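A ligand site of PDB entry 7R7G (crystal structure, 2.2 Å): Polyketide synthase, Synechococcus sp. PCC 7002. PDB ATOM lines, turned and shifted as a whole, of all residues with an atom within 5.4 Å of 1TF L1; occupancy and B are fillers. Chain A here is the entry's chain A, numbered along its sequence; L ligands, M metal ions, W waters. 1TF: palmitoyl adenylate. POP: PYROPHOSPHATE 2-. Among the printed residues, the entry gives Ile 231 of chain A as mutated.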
ATOM      1  N   THR A 171     -40.095 -14.092  30.795  1.00  0.00           N
ATOM      2  CA  THR A 171     -39.583 -14.868  29.651  1.00  0.00           C
ATOM      3  C   THR A 171     -39.609 -13.981  28.417  1.00  0.00           C
ATOM      4  O   THR A 171     -40.379 -13.036  28.397  1.00  0.00           O
ATOM      5  CB  THR A 171     -40.357 -16.187  29.526  1.00  0.00           C
ATOM      6  OG1 THR A 171     -41.698 -15.924  29.131  1.00  0.00           O
ATOM      7  CG2 THR A 171     -40.352 -16.981  30.810  1.00  0.00           C
ATOM      8  N   SER A 172     -38.829 -14.329  27.394  1.00  0.00           N
ATOM      9  CA  SER A 172     -38.725 -13.516  26.159  1.00  0.00           C
ATOM     10  C   SER A 172     -40.057 -13.464  25.391  1.00  0.00           C
ATOM     11  O   SER A 172     -40.283 -12.460  24.717  1.00  0.00           O
ATOM     12  CB  SER A 172     -37.625 -14.029  25.307  1.00  0.00           C
ATOM     13  OG  SER A 172     -38.001 -15.247  24.679  1.00  0.00           O
ATOM     14  N   ILE A 195     -22.890 -21.288  38.913  1.00  0.00           N
ATOM     15  CA  ILE A 195     -22.076 -20.639  37.847  1.00  0.00           C
ATOM     16  C   ILE A 195     -20.599 -20.686  38.260  1.00  0.00           C
ATOM     17  O   ILE A 195     -19.775 -20.878  37.383  1.00  0.00           O
ATOM     18  CB  ILE A 195     -22.554 -19.192  37.596  1.00  0.00           C
ATOM     19  CG1 ILE A 195     -24.034 -19.148  37.191  1.00  0.00           C
ATOM     20  CG2 ILE A 195     -21.685 -18.480  36.589  1.00  0.00           C
ATOM     21  CD1 ILE A 195     -24.552 -17.762  36.907  1.00  0.00           C
ATOM     22  N   PHE A 199     -17.599 -22.132  36.217  1.00  0.00           N
ATOM     23  CA  PHE A 199     -16.677 -21.134  35.638  1.00  0.00           C
ATOM     24  C   PHE A 199     -15.338 -21.176  36.378  1.00  0.00           C
ATOM     25  O   PHE A 199     -14.323 -20.908  35.756  1.00  0.00           O
ATOM     26  CB  PHE A 199     -17.320 -19.759  35.645  1.00  0.00           C
ATOM     27  CG  PHE A 199     -18.297 -19.504  34.532  1.00  0.00           C
ATOM     28  CD1 PHE A 199     -19.132 -20.518  34.073  1.00  0.00           C
ATOM     29  CD2 PHE A 199     -18.376 -18.267  33.930  1.00  0.00           C
ATOM     30  CE1 PHE A 199     -20.030 -20.287  33.051  1.00  0.00           C
ATOM     31  CE2 PHE A 199     -19.268 -18.045  32.895  1.00  0.00           C
ATOM     32  CZ  PHE A 199     -20.098 -19.051  32.462  1.00  0.00           C
ATOM     33  N   ASP A 201     -14.152 -19.104  38.554  1.00  0.00           N
ATOM     34  CA  ASP A 201     -13.529 -17.762  38.535  1.00  0.00           C
ATOM     35  C   ASP A 201     -12.978 -17.428  39.921  1.00  0.00           C
ATOM     36  O   ASP A 201     -13.442 -18.014  40.899  1.00  0.00           O
ATOM     37  CB  ASP A 201     -14.466 -16.690  38.009  1.00  0.00           C
ATOM     38  CG  ASP A 201     -14.529 -16.605  36.493  1.00  0.00           C
ATOM     39  OD1 ASP A 201     -13.482 -16.801  35.853  1.00  0.00           O
ATOM     40  OD2 ASP A 201     -15.627 -16.346  35.976  1.00  0.00           O
ATOM     41  N   ASP A 216     -31.722 -12.860  31.955  1.00  0.00           N
ATOM     42  CA  ASP A 216     -30.812 -14.028  31.823  1.00  0.00           C
ATOM     43  C   ASP A 216     -29.319 -13.744  31.955  1.00  0.00           C
ATOM     44  O   ASP A 216     -28.920 -13.150  32.987  1.00  0.00           O
ATOM     45  CB  ASP A 216     -31.161 -14.892  30.596  1.00  0.00           C
ATOM     46  CG  ASP A 216     -31.312 -14.134  29.291  1.00  0.00           C
ATOM     47  OD1 ASP A 216     -30.284 -13.703  28.743  1.00  0.00           O
ATOM     48  OD2 ASP A 216     -32.465 -13.970  28.845  1.00  0.00           O
ATOM     49  N   MET A 217     -28.518 -14.185  30.980  1.00  0.00           N
ATOM     50  CA  MET A 217     -27.042 -14.104  31.066  1.00  0.00           C
ATOM     51  C   MET A 217     -26.564 -12.696  31.417  1.00  0.00           C
ATOM     52  O   MET A 217     -25.559 -12.589  32.130  1.00  0.00           O
ATOM     53  CB  MET A 217     -26.452 -14.562  29.730  1.00  0.00           C
ATOM     54  CG  MET A 217     -27.014 -15.885  29.256  1.00  0.00           C
ATOM     55  SD  MET A 217     -26.016 -16.667  27.958  1.00  0.00           S
ATOM     56  CE  MET A 217     -25.988 -15.348  26.743  1.00  0.00           C
ATOM     57  N   GLY A 221     -25.671 -13.150  35.393  1.00  0.00           N
ATOM     58  CA  GLY A 221     -24.273 -13.461  35.060  1.00  0.00           C
ATOM     59  C   GLY A 221     -23.460 -12.222  34.803  1.00  0.00           C
ATOM     60  O   GLY A 221     -22.331 -12.173  35.277  1.00  0.00           O
ATOM     61  N   GLY A 222     -24.019 -11.243  34.127  1.00  0.00           N
ATOM     62  CA  GLY A 222     -23.265 -10.021  33.804  1.00  0.00           C
ATOM     63  C   GLY A 222     -23.255  -9.034  34.938  1.00  0.00           C
ATOM     64  O   GLY A 222     -22.364  -8.202  34.961  1.00  0.00           O
ATOM     65  N   GLN A 225     -23.007 -12.141  39.095  1.00  0.00           N
ATOM     66  CA  GLN A 225     -21.825 -13.029  39.251  1.00  0.00           C
ATOM     67  C   GLN A 225     -20.554 -12.236  39.552  1.00  0.00           C
ATOM     68  O   GLN A 225     -19.788 -12.681  40.404  1.00  0.00           O
ATOM     69  CB  GLN A 225     -21.666 -14.019  38.085  1.00  0.00           C
ATOM     70  CG  GLN A 225     -20.536 -15.016  38.264  1.00  0.00           C
ATOM     71  CD  GLN A 225     -20.817 -16.092  39.277  1.00  0.00           C
ATOM     72  OE1 GLN A 225     -19.959 -16.917  39.575  1.00  0.00           O
ATOM     73  NE2 GLN A 225     -22.009 -16.093  39.827  1.00  0.00           N
ATOM     74  N   PRO A 226     -20.262 -11.077  38.902  1.00  0.00           N
ATOM     75  CA  PRO A 226     -19.156 -10.219  39.335  1.00  0.00           C
ATOM     76  C   PRO A 226     -19.202  -9.935  40.845  1.00  0.00           C
ATOM     77  O   PRO A 226     -18.209 -10.095  41.479  1.00  0.00           O
ATOM     78  CB  PRO A 226     -19.395  -8.956  38.521  1.00  0.00           C
ATOM     79  CG  PRO A 226     -19.853  -9.487  37.209  1.00  0.00           C
ATOM     80  CD  PRO A 226     -20.815 -10.567  37.626  1.00  0.00           C
ATOM     81  N   ILE A 231     -15.137  -9.373  41.647  1.00  0.00           N
ATOM     82  CA  ILE A 231     -14.248  -9.128  40.475  1.00  0.00           C
ATOM     83  C   ILE A 231     -14.684  -7.848  39.778  1.00  0.00           C
ATOM     84  O   ILE A 231     -15.774  -7.337  40.093  1.00  0.00           O
ATOM     85  CB  ILE A 231     -14.258 -10.320  39.497  1.00  0.00           C
ATOM     86  CG1 ILE A 231     -15.647 -10.590  38.926  1.00  0.00           C
ATOM     87  CG2 ILE A 231     -13.660 -11.561  40.143  1.00  0.00           C
ATOM     88  CD1 ILE A 231     -15.664 -11.604  37.802  1.00  0.00           C
ATOM     89  N   GLN A 233     -15.980  -5.999  36.488  1.00  0.00           N
ATOM     90  CA  GLN A 233     -16.676  -6.293  35.231  1.00  0.00           C
ATOM     91  C   GLN A 233     -16.662  -5.072  34.328  1.00  0.00           C
ATOM     92  O   GLN A 233     -16.966  -3.998  34.825  1.00  0.00           O
ATOM     93  CB  GLN A 233     -18.111  -6.724  35.534  1.00  0.00           C
ATOM     94  CG  GLN A 233     -18.931  -7.072  34.311  1.00  0.00           C
ATOM     95  CD  GLN A 233     -18.490  -8.356  33.666  1.00  0.00           C
ATOM     96  OE1 GLN A 233     -18.316  -8.428  32.455  1.00  0.00           O
ATOM     97  NE2 GLN A 233     -18.281  -9.382  34.470  1.00  0.00           N
ATOM     98  N   THR A 259     -12.985 -14.138  31.442  1.00  0.00           N
ATOM     99  CA  THR A 259     -14.310 -14.741  31.273  1.00  0.00           C
ATOM    100  C   THR A 259     -15.306 -13.814  30.578  1.00  0.00           C
ATOM    101  O   THR A 259     -15.746 -12.863  31.222  1.00  0.00           O
ATOM    102  CB  THR A 259     -14.835 -15.137  32.655  1.00  0.00           C
ATOM    103  OG1 THR A 259     -13.730 -15.569  33.451  1.00  0.00           O
ATOM    104  CG2 THR A 259     -15.891 -16.210  32.597  1.00  0.00           C
ATOM    105  N   PHE A 291     -18.020 -18.561  27.209  1.00  0.00           N
ATOM    106  CA  PHE A 291     -19.317 -19.274  27.326  1.00  0.00           C
ATOM    107  C   PHE A 291     -20.242 -19.071  26.121  1.00  0.00           C
ATOM    108  O   PHE A 291     -20.184 -18.005  25.493  1.00  0.00           O
ATOM    109  CB  PHE A 291     -19.987 -19.001  28.682  1.00  0.00           C
ATOM    110  CG  PHE A 291     -20.498 -17.602  28.943  1.00  0.00           C
ATOM    111  CD1 PHE A 291     -21.740 -17.198  28.484  1.00  0.00           C
ATOM    112  CD2 PHE A 291     -19.751 -16.706  29.698  1.00  0.00           C
ATOM    113  CE1 PHE A 291     -22.214 -15.923  28.753  1.00  0.00           C
ATOM    114  CE2 PHE A 291     -20.231 -15.438  29.963  1.00  0.00           C
ATOM    115  CZ  PHE A 291     -21.458 -15.049  29.491  1.00  0.00           C
ATOM    116  N   SER A 292     -21.107 -20.050  25.854  1.00  0.00           N
ATOM    117  CA  SER A 292     -22.115 -19.910  24.768  1.00  0.00           C
ATOM    118  C   SER A 292     -23.452 -20.456  25.255  1.00  0.00           C
ATOM    119  O   SER A 292     -23.522 -21.674  25.526  1.00  0.00           O
ATOM    120  CB  SER A 292     -21.665 -20.604  23.505  1.00  0.00           C
ATOM    121  OG  SER A 292     -22.611 -20.390  22.475  1.00  0.00           O
ATOM    122  N   GLY A 293     -24.468 -19.600  25.386  1.00  0.00           N
ATOM    123  CA  GLY A 293     -25.763 -20.047  25.954  1.00  0.00           C
ATOM    124  C   GLY A 293     -26.934 -19.225  25.447  1.00  0.00           C
ATOM    125  O   GLY A 293     -26.667 -18.265  24.706  1.00  0.00           O
ATOM    126  N   ALA A 294     -28.169 -19.648  25.754  1.00  0.00           N
ATOM    127  CA  ALA A 294     -29.400 -18.927  25.358  1.00  0.00           C
ATOM    128  C   ALA A 294     -29.740 -19.171  23.887  1.00  0.00           C
ATOM    129  O   ALA A 294     -30.629 -18.469  23.371  1.00  0.00           O
ATOM    130  CB  ALA A 294     -29.325 -17.452  25.699  1.00  0.00           C
ATOM    131  N   GLU A 295     -29.083 -20.141  23.252  1.00  0.00           N
ATOM    132  CA  GLU A 295     -29.311 -20.397  21.808  1.00  0.00           C
ATOM    133  C   GLU A 295     -28.611 -21.704  21.391  1.00  0.00           C
ATOM    134  O   GLU A 295     -27.506 -21.934  21.920  1.00  0.00           O
ATOM    135  CB  GLU A 295     -28.722 -19.238  20.987  1.00  0.00           C
ATOM    136  CG  GLU A 295     -29.111 -19.253  19.520  1.00  0.00           C
ATOM    137  CD  GLU A 295     -28.411 -18.216  18.663  1.00  0.00           C
ATOM    138  OE1 GLU A 295     -27.449 -17.599  19.155  1.00  0.00           O
ATOM    139  OE2 GLU A 295     -28.832 -18.021  17.507  1.00  0.00           O
ATOM    140  N   PRO A 296     -29.169 -22.578  20.509  1.00  0.00           N
ATOM    141  CA  PRO A 296     -28.419 -23.742  20.037  1.00  0.00           C
ATOM    142  C   PRO A 296     -26.938 -23.474  19.709  1.00  0.00           C
ATOM    143  O   PRO A 296     -26.657 -22.602  18.918  1.00  0.00           O
ATOM    144  CB  PRO A 296     -29.145 -24.098  18.738  1.00  0.00           C
ATOM    145  CG  PRO A 296     -30.587 -23.747  19.029  1.00  0.00           C
ATOM    146  CD  PRO A 296     -30.499 -22.500  19.884  1.00  0.00           C
ATOM    147  N   ILE A 297     -26.027 -24.247  20.327  1.00  0.00           N
ATOM    148  CA  ILE A 297     -24.576 -24.128  19.990  1.00  0.00           C
ATOM    149  C   ILE A 297     -24.330 -24.943  18.714  1.00  0.00           C
ATOM    150  O   ILE A 297     -24.625 -26.143  18.722  1.00  0.00           O
ATOM    151  CB  ILE A 297     -23.686 -24.542  21.185  1.00  0.00           C
ATOM    152  CG1 ILE A 297     -23.983 -23.714  22.429  1.00  0.00           C
ATOM    153  CG2 ILE A 297     -22.219 -24.489  20.807  1.00  0.00           C
ATOM    154  CD1 ILE A 297     -24.215 -24.536  23.671  1.00  0.00           C
ATOM    155  N   CYS A 322     -23.090 -23.986  27.660  1.00  0.00           N
ATOM    156  CA  CYS A 322     -23.937 -23.921  28.869  1.00  0.00           C
ATOM    157  C   CYS A 322     -25.412 -23.940  28.476  1.00  0.00           C
ATOM    158  O   CYS A 322     -25.726 -23.446  27.393  1.00  0.00           O
ATOM    159  CB  CYS A 322     -23.622 -22.663  29.692  1.00  0.00           C
ATOM    160  SG  CYS A 322     -23.386 -21.158  28.724  1.00  0.00           S
ATOM    161  N   TYR A 323     -26.264 -24.458  29.349  1.00  0.00           N
ATOM    162  CA  TYR A 323     -27.720 -24.445  29.116  1.00  0.00           C
ATOM    163  C   TYR A 323     -28.452 -24.001  30.364  1.00  0.00           C
ATOM    164  O   TYR A 323     -28.025 -24.366  31.459  1.00  0.00           O
ATOM    165  CB  TYR A 323     -28.267 -25.814  28.684  1.00  0.00           C
ATOM    166  CG  TYR A 323     -29.739 -26.057  28.859  1.00  0.00           C
ATOM    167  CD1 TYR A 323     -30.660 -25.538  27.969  1.00  0.00           C
ATOM    168  CD2 TYR A 323     -30.217 -26.837  29.893  1.00  0.00           C
ATOM    169  CE1 TYR A 323     -32.021 -25.760  28.116  1.00  0.00           C
ATOM    170  CE2 TYR A 323     -31.572 -27.085  30.055  1.00  0.00           C
ATOM    171  CZ  TYR A 323     -32.478 -26.544  29.155  1.00  0.00           C
ATOM    172  OH  TYR A 323     -33.808 -26.776  29.308  1.00  0.00           O
ATOM    173  N   GLY A 324     -29.554 -23.280  30.169  1.00  0.00           N
ATOM    174  CA  GLY A 324     -30.410 -22.897  31.294  1.00  0.00           C
ATOM    175  C   GLY A 324     -31.586 -22.081  30.827  1.00  0.00           C
ATOM    176  O   GLY A 324     -31.681 -21.820  29.631  1.00  0.00           O
ATOM    177  N   MET A 325     -32.453 -21.704  31.760  1.00  0.00           N
ATOM    178  CA  MET A 325     -33.614 -20.843  31.457  1.00  0.00           C
ATOM    179  C   MET A 325     -33.937 -19.966  32.668  1.00  0.00           C
ATOM    180  O   MET A 325     -33.282 -20.126  33.693  1.00  0.00           O
ATOM    181  CB  MET A 325     -34.845 -21.702  31.155  1.00  0.00           C
ATOM    182  CG  MET A 325     -35.174 -22.669  32.249  1.00  0.00           C
ATOM    183  SD  MET A 325     -35.758 -24.224  31.596  1.00  0.00           S
ATOM    184  CE  MET A 325     -37.213 -23.650  30.732  1.00  0.00           C
ATOM    185  N   ALA A 326     -34.978 -19.136  32.563  1.00  0.00           N
ATOM    186  CA  ALA A 326     -35.397 -18.261  33.681  1.00  0.00           C
ATOM    187  C   ALA A 326     -36.053 -19.068  34.789  1.00  0.00           C
ATOM    188  O   ALA A 326     -35.879 -18.688  35.955  1.00  0.00           O
ATOM    189  CB  ALA A 326     -36.311 -17.210  33.142  1.00  0.00           C
ATOM    190  N   GLU A 327     -36.757 -20.151  34.439  1.00  0.00           N
ATOM    191  CA  GLU A 327     -37.438 -21.016  35.442  1.00  0.00           C
ATOM    192  C   GLU A 327     -36.378 -21.741  36.272  1.00  0.00           C
ATOM    193  O   GLU A 327     -36.721 -22.254  37.354  1.00  0.00           O
ATOM    194  CB  GLU A 327     -38.377 -21.995  34.736  1.00  0.00           C
ATOM    195  CG  GLU A 327     -39.570 -21.333  34.065  1.00  0.00           C
ATOM    196  CD  GLU A 327     -39.325 -20.727  32.693  1.00  0.00           C
ATOM    197  OE1 GLU A 327     -38.192 -20.829  32.188  1.00  0.00           O
ATOM    198  OE2 GLU A 327     -40.268 -20.158  32.124  1.00  0.00           O
ATOM    199  N   LEU A 330     -30.842 -19.362  36.166  1.00  0.00           N
ATOM    200  CA  LEU A 330     -29.979 -19.120  34.986  1.00  0.00           C
ATOM    201  C   LEU A 330     -29.353 -20.414  34.443  1.00  0.00           C
ATOM    202  O   LEU A 330     -29.766 -20.820  33.355  1.00  0.00           O
ATOM    203  CB  LEU A 330     -28.897 -18.071  35.295  1.00  0.00           C
ATOM    204  CG  LEU A 330     -28.043 -17.667  34.095  1.00  0.00           C
ATOM    205  CD1 LEU A 330     -28.916 -17.247  32.918  1.00  0.00           C
ATOM    206  CD2 LEU A 330     -27.059 -16.565  34.451  1.00  0.00           C
ATOM    207  N   ILE A 331     -28.397 -21.029  35.153  1.00  0.00           N
ATOM    208  CA  ILE A 331     -27.673 -22.201  34.583  1.00  0.00           C
ATOM    209  C   ILE A 331     -28.160 -23.556  35.130  1.00  0.00           C
ATOM    210  O   ILE A 331     -28.715 -23.583  36.242  1.00  0.00           O
ATOM    211  CB  ILE A 331     -26.148 -22.046  34.765  1.00  0.00           C
ATOM    212  CG1 ILE A 331     -25.356 -22.801  33.695  1.00  0.00           C
ATOM    213  CG2 ILE A 331     -25.700 -22.423  36.170  1.00  0.00           C
ATOM    214  CD1 ILE A 331     -23.896 -22.431  33.640  1.00  0.00           C
ATOM    215  N   SER A 372     -24.423 -29.310  25.661  1.00  0.00           N
ATOM    216  CA  SER A 372     -24.682 -28.025  26.345  1.00  0.00           C
ATOM    217  C   SER A 372     -24.119 -28.112  27.757  1.00  0.00           C
ATOM    218  O   SER A 372     -24.563 -27.335  28.601  1.00  0.00           O
ATOM    219  CB  SER A 372     -26.133 -27.630  26.254  1.00  0.00           C
ATOM    220  OG  SER A 372     -26.402 -27.077  24.985  1.00  0.00           O
ATOM    221  N   THR A 435     -39.165 -28.160  31.380  1.00  0.00           N
ATOM    222  CA  THR A 435     -38.503 -27.013  30.706  1.00  0.00           C
ATOM    223  C   THR A 435     -39.207 -26.706  29.381  1.00  0.00           C
ATOM    224  O   THR A 435     -39.079 -25.569  28.898  1.00  0.00           O
ATOM    225  CB  THR A 435     -37.027 -27.348  30.464  1.00  0.00           C
ATOM    226  OG1 THR A 435     -36.976 -28.433  29.530  1.00  0.00           O
ATOM    227  CG2 THR A 435     -36.306 -27.740  31.730  1.00  0.00           C
ATOM    228  N   ASP A 437     -38.258 -28.076  26.853  1.00  0.00           N
ATOM    229  CA  ASP A 437     -37.122 -28.258  25.912  1.00  0.00           C
ATOM    230  C   ASP A 437     -36.910 -29.753  25.687  1.00  0.00           C
ATOM    231  O   ASP A 437     -36.913 -30.499  26.679  1.00  0.00           O
ATOM    232  CB  ASP A 437     -35.837 -27.629  26.443  1.00  0.00           C
ATOM    233  CG  ASP A 437     -35.933 -26.126  26.582  1.00  0.00           C
ATOM    234  OD1 ASP A 437     -36.101 -25.454  25.549  1.00  0.00           O
ATOM    235  OD2 ASP A 437     -35.841 -25.637  27.721  1.00  0.00           O
ATOM    236  N   ILE A 448     -29.328 -30.618  23.682  1.00  0.00           N
ATOM    237  CA  ILE A 448     -30.657 -29.960  23.545  1.00  0.00           C
ATOM    238  C   ILE A 448     -31.000 -29.980  22.056  1.00  0.00           C
ATOM    239  O   ILE A 448     -30.186 -29.532  21.257  1.00  0.00           O
ATOM    240  CB  ILE A 448     -30.723 -28.555  24.184  1.00  0.00           C
ATOM    241  CG1 ILE A 448     -30.397 -28.578  25.674  1.00  0.00           C
ATOM    242  CG2 ILE A 448     -32.061 -27.897  23.912  1.00  0.00           C
ATOM    243  CD1 ILE A 448     -31.557 -28.997  26.531  1.00  0.00           C
ATOM    244  N   ARG A 451     -37.288 -26.864  21.172  1.00  0.00           N
ATOM    245  CA  ARG A 451     -38.451 -26.547  22.023  1.00  0.00           C
ATOM    246  C   ARG A 451     -39.656 -27.375  21.585  1.00  0.00           C
ATOM    247  O   ARG A 451     -39.897 -27.448  20.380  1.00  0.00           O
ATOM    248  CB  ARG A 451     -38.755 -25.056  21.935  1.00  0.00           C
ATOM    249  CG  ARG A 451     -37.562 -24.147  22.169  1.00  0.00           C
ATOM    250  CD  ARG A 451     -38.061 -22.827  22.723  1.00  0.00           C
ATOM    251  NE  ARG A 451     -37.229 -21.687  22.381  1.00  0.00           N
ATOM    252  CZ  ARG A 451     -36.914 -20.727  23.237  1.00  0.00           C
ATOM    253  NH1 ARG A 451     -37.372 -20.784  24.476  1.00  0.00           N
ATOM    254  NH2 ARG A 451     -36.163 -19.722  22.856  1.00  0.00           N
ATOM    255  N   LYS A 550     -35.149 -12.718  19.573  1.00  0.00           N
ATOM    256  CA  LYS A 550     -35.572 -14.112  19.319  1.00  0.00           C
ATOM    257  C   LYS A 550     -36.851 -14.110  18.482  1.00  0.00           C
ATOM    258  O   LYS A 550     -37.792 -13.418  18.839  1.00  0.00           O
ATOM    259  CB  LYS A 550     -35.811 -14.872  20.625  1.00  0.00           C
ATOM    260  CG  LYS A 550     -34.591 -15.476  21.303  1.00  0.00           C
ATOM    261  CD  LYS A 550     -34.898 -15.907  22.721  1.00  0.00           C
ATOM    262  CE  LYS A 550     -33.791 -16.729  23.354  1.00  0.00           C
ATOM    263  NZ  LYS A 550     -33.967 -16.846  24.813  1.00  0.00           N
HETATM  264  C15 1TF L   1     -30.995 -18.535  29.748  1.00  0.00           C
HETATM  265  C17 1TF L   1     -28.893 -19.862  30.074  1.00  0.00           C
HETATM  266  C20 1TF L   1     -25.870 -19.174  30.821  1.00  0.00           C
HETATM  267  C21 1TF L   1     -24.891 -19.178  31.981  1.00  0.00           C
HETATM  268  C22 1TF L   1     -23.635 -18.372  31.677  1.00  0.00           C
HETATM  269  C24 1TF L   1     -22.702 -16.787  33.407  1.00  0.00           C
HETATM  270  C26 1TF L   1     -20.930 -15.261  34.412  1.00  0.00           C
HETATM  271  C28 1TF L   1     -18.599 -14.354  34.817  1.00  0.00           C
HETATM  272  C02 1TF L   1     -28.770 -24.232  24.690  1.00  0.00           C
HETATM  273  C03 1TF L   1     -29.725 -23.344  25.213  1.00  0.00           C
HETATM  274  C04 1TF L   1     -30.915 -23.206  24.549  1.00  0.00           C
HETATM  275  C06 1TF L   1     -32.977 -21.887  24.858  1.00  0.00           C
HETATM  276  C08 1TF L   1     -34.529 -21.194  26.443  1.00  0.00           C
HETATM  277  C09 1TF L   1     -34.541 -20.325  27.672  1.00  0.00           C
HETATM  278  C14 1TF L   1     -32.063 -18.198  28.718  1.00  0.00           C
HETATM  279  C16 1TF L   1     -29.741 -19.082  29.080  1.00  0.00           C
HETATM  280  C18 1TF L   1     -27.603 -20.407  29.505  1.00  0.00           C
HETATM  281  C19 1TF L   1     -26.572 -20.514  30.620  1.00  0.00           C
HETATM  282  C23 1TF L   1     -23.674 -16.966  32.258  1.00  0.00           C
HETATM  283  C25 1TF L   1     -21.854 -15.530  33.244  1.00  0.00           C
HETATM  284  C27 1TF L   1     -19.945 -14.143  34.115  1.00  0.00           C
HETATM  285  C29 1TF L   1     -18.232 -13.209  35.755  1.00  0.00           C
HETATM  286  C32 1TF L   1     -34.252 -22.401  26.771  1.00  0.00           C
HETATM  287  C34 1TF L   1     -33.916 -22.982  25.419  1.00  0.00           C
HETATM  288  C36 1TF L   1     -30.917 -21.936  26.290  1.00  0.00           C
HETATM  289  C39 1TF L   1     -30.213 -24.725  22.977  1.00  0.00           C
HETATM  290  N01 1TF L   1     -27.503 -24.434  25.351  1.00  0.00           N
HETATM  291  N05 1TF L   1     -31.617 -22.317  25.242  1.00  0.00           N
HETATM  292  N37 1TF L   1     -29.759 -22.547  26.288  1.00  0.00           N
HETATM  293  N38 1TF L   1     -31.114 -23.903  23.436  1.00  0.00           N
HETATM  294  N40 1TF L   1     -29.054 -24.892  23.588  1.00  0.00           N
HETATM  295  O07 1TF L   1     -33.325 -20.806  25.444  1.00  0.00           O
HETATM  296  O10 1TF L   1     -34.612 -18.998  27.258  1.00  0.00           O
HETATM  297  O12 1TF L   1     -35.161 -16.555  27.791  1.00  0.00           O
HETATM  298  O13 1TF L   1     -33.233 -17.520  29.093  1.00  0.00           O
HETATM  299  O30 1TF L   1     -31.854 -18.514  27.592  1.00  0.00           O
HETATM  300  O31 1TF L   1     -35.683 -18.274  29.471  1.00  0.00           O
HETATM  301  O33 1TF L   1     -35.445 -23.052  27.391  1.00  0.00           O
HETATM  302  O35 1TF L   1     -35.032 -23.075  24.647  1.00  0.00           O
HETATM  303  P11 1TF L   1     -34.701 -17.838  28.417  1.00  0.00           P
HETATM  304  P1  POP L   2     -40.710 -18.177  26.422  1.00  0.00           P
HETATM  305  O1  POP L   2     -41.342 -16.848  26.668  1.00  0.00           O
HETATM  306  O2  POP L   2     -41.358 -18.906  25.316  1.00  0.00           O
HETATM  307  O3  POP L   2     -40.574 -18.993  27.658  1.00  0.00           O
HETATM  308  O   POP L   2     -39.243 -17.902  25.883  1.00  0.00           O
HETATM  309  P2  POP L   2     -37.821 -18.179  26.538  1.00  0.00           P
HETATM  310  O4  POP L   2     -37.812 -17.245  27.697  1.00  0.00           O
HETATM  311  O5  POP L   2     -36.816 -17.851  25.484  1.00  0.00           O
HETATM  312  O6  POP L   2     -37.792 -19.619  26.943  1.00  0.00           O
HETATM  313 MG    MG M   1     -39.575 -20.840  27.587  1.00  0.00          MG
HETATM  314  O   HOH W   1     -38.126 -20.048  29.543  1.00  0.00           O
HETATM  315  O   HOH W   2     -37.929 -22.108  27.864  1.00  0.00           O
HETATM  316  O   HOH W   3     -27.557 -26.696  21.702  1.00  0.00           O
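An oxygen (O4) of POP L2 lies close to an oxygen (O12) of 1TF L1 (2.7 Å).
N of Ile 231 is in hydrogen-bond range of O of Pro 226.
The backbone NH (N) of Tyr 323 lies within hydrogen-bond range of the backbone carbonyl oxygen (O) of Ser 372 (3.4 Å).
The side-chain hydroxyl (OG1) of Thr 435 is in hydrogen-bond range of the backbone NH (N) of Asp 437.
OG1 of Thr 259 lies within hydrogen-bond range of OD1 of Asp 201 (2.7 Å).
The backbone NH of Cys 322 is in hydrogen-bond range of the backbone carbonyl oxygen of Ser 292 (3.2 Å).
OH of Tyr 323 sits at hydrogen-bond distance from OD2 of Asp 437 (2.8 Å).
The backbone NH of Met 325 is in hydrogen-bond range of the backbone carbonyl oxygen of Leu 330.
N of Gly 222 is in hydrogen-bond range of O of Met 217 (2.9 Å).
Water W3 bridges N40 of 1TF L1 (3.0 Å) and N of Ile 297 (3.2 Å).
Water W1 lies within hydrogen-bond range of the side-chain carboxylate of Glu 327 (2.8 Å), an oxygen (O31) of 1TF L1 (3.0 Å) and an oxygen (O4) of POP L2 (3.4 Å).
The backbone NH (N) of Ser 172 lies within hydrogen-bond range of an oxygen (O4) of POP L2, at 3.1 Å.
A nitrogen (N01) of 1TF L1 is in hydrogen-bond range of the backbone carbonyl oxygen (O) of Cys 322, at 2.9 Å.
The side-chain hydroxyl (OG1) of Thr 171 is in hydrogen-bond range of an oxygen (O1) of POP L2 (2.7 Å).
An oxygen (O31) of 1TF L1 lies within hydrogen-bond range of the backbone NH (N) of Ala 326, 3.3 Å away.
N01 of 1TF L1 is in hydrogen-bond range of OG of Ser 372 (2.9 Å).
O35 of 1TF L1 sits at hydrogen-bond distance from NH1 of Arg 451.
The side-chain amino group (NZ) of Lys 550 lies within salt-bridge range of an oxygen (O5) of POP L2 (3.1 Å).
O33 of 1TF L1 sits at hydrogen-bond distance from OD2 of Asp 437 (2.6 Å).
O12 of 1TF L1 is in salt-bridge range of NZ of Lys 550 (3.2 Å).
OG of Ser 172 is in hydrogen-bond range of O5 of POP L2 (3.0 Å).
N37 of 1TF L1 sits at hydrogen-bond distance from N of Ala 294, 3.3 Å away.
The guanidinium group (NH1) of Arg 451 lies within salt-bridge range of an oxygen (O5) of POP L2 (3.2 Å).
Merely in contact with 1TF L1: Ile 195 (3.7 Å), Phe 199 (3.6 Å), Asp 201 (3.8 Å), Asp 216 (3.6 Å), Met 217 (3.8 Å), Gly 221 (3.3 Å), Gln 225 (3.9 Å), Ile 231 (3.7 Å), Thr 259 (3.96 Å), Phe 291 (3.7 Å), Glu 295 (3.7 Å), Pro 296 (3.4 Å), Ile 297 (3.7 Å), Tyr 323 (3.5 Å), Gly 324 (3.4 Å), Met 325 (3.8 Å), Leu 330 (3.5 Å), Ile 331 (3.8 Å) and Ile 448 (3.8 Å).
Hydrophobic or aromatic side chains within 4 Å of 1TF L1: Ile 195, Phe 199, Met 217, Ile 231, Phe 291, Ala 294, Pro 296, Ile 297, Tyr 323, Met 325, Ala 326, Leu 330, Ile 331 and Ile 448.
Within 4 Å of 1TF L1: Ile 195, Phe 199, Asp 201, Asp 216, Met 217, Gly 221, Gln 225, Ile 231, Thr 259, Phe 291, Ala 294, Glu 295, Pro 296, Ile 297, Cys 322, Tyr 323, Gly 324, Met 325, Ala 326, Leu 330, Ile 331, Ser 372, Asp 437, Ile 448, Arg 451 and Lys 550.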
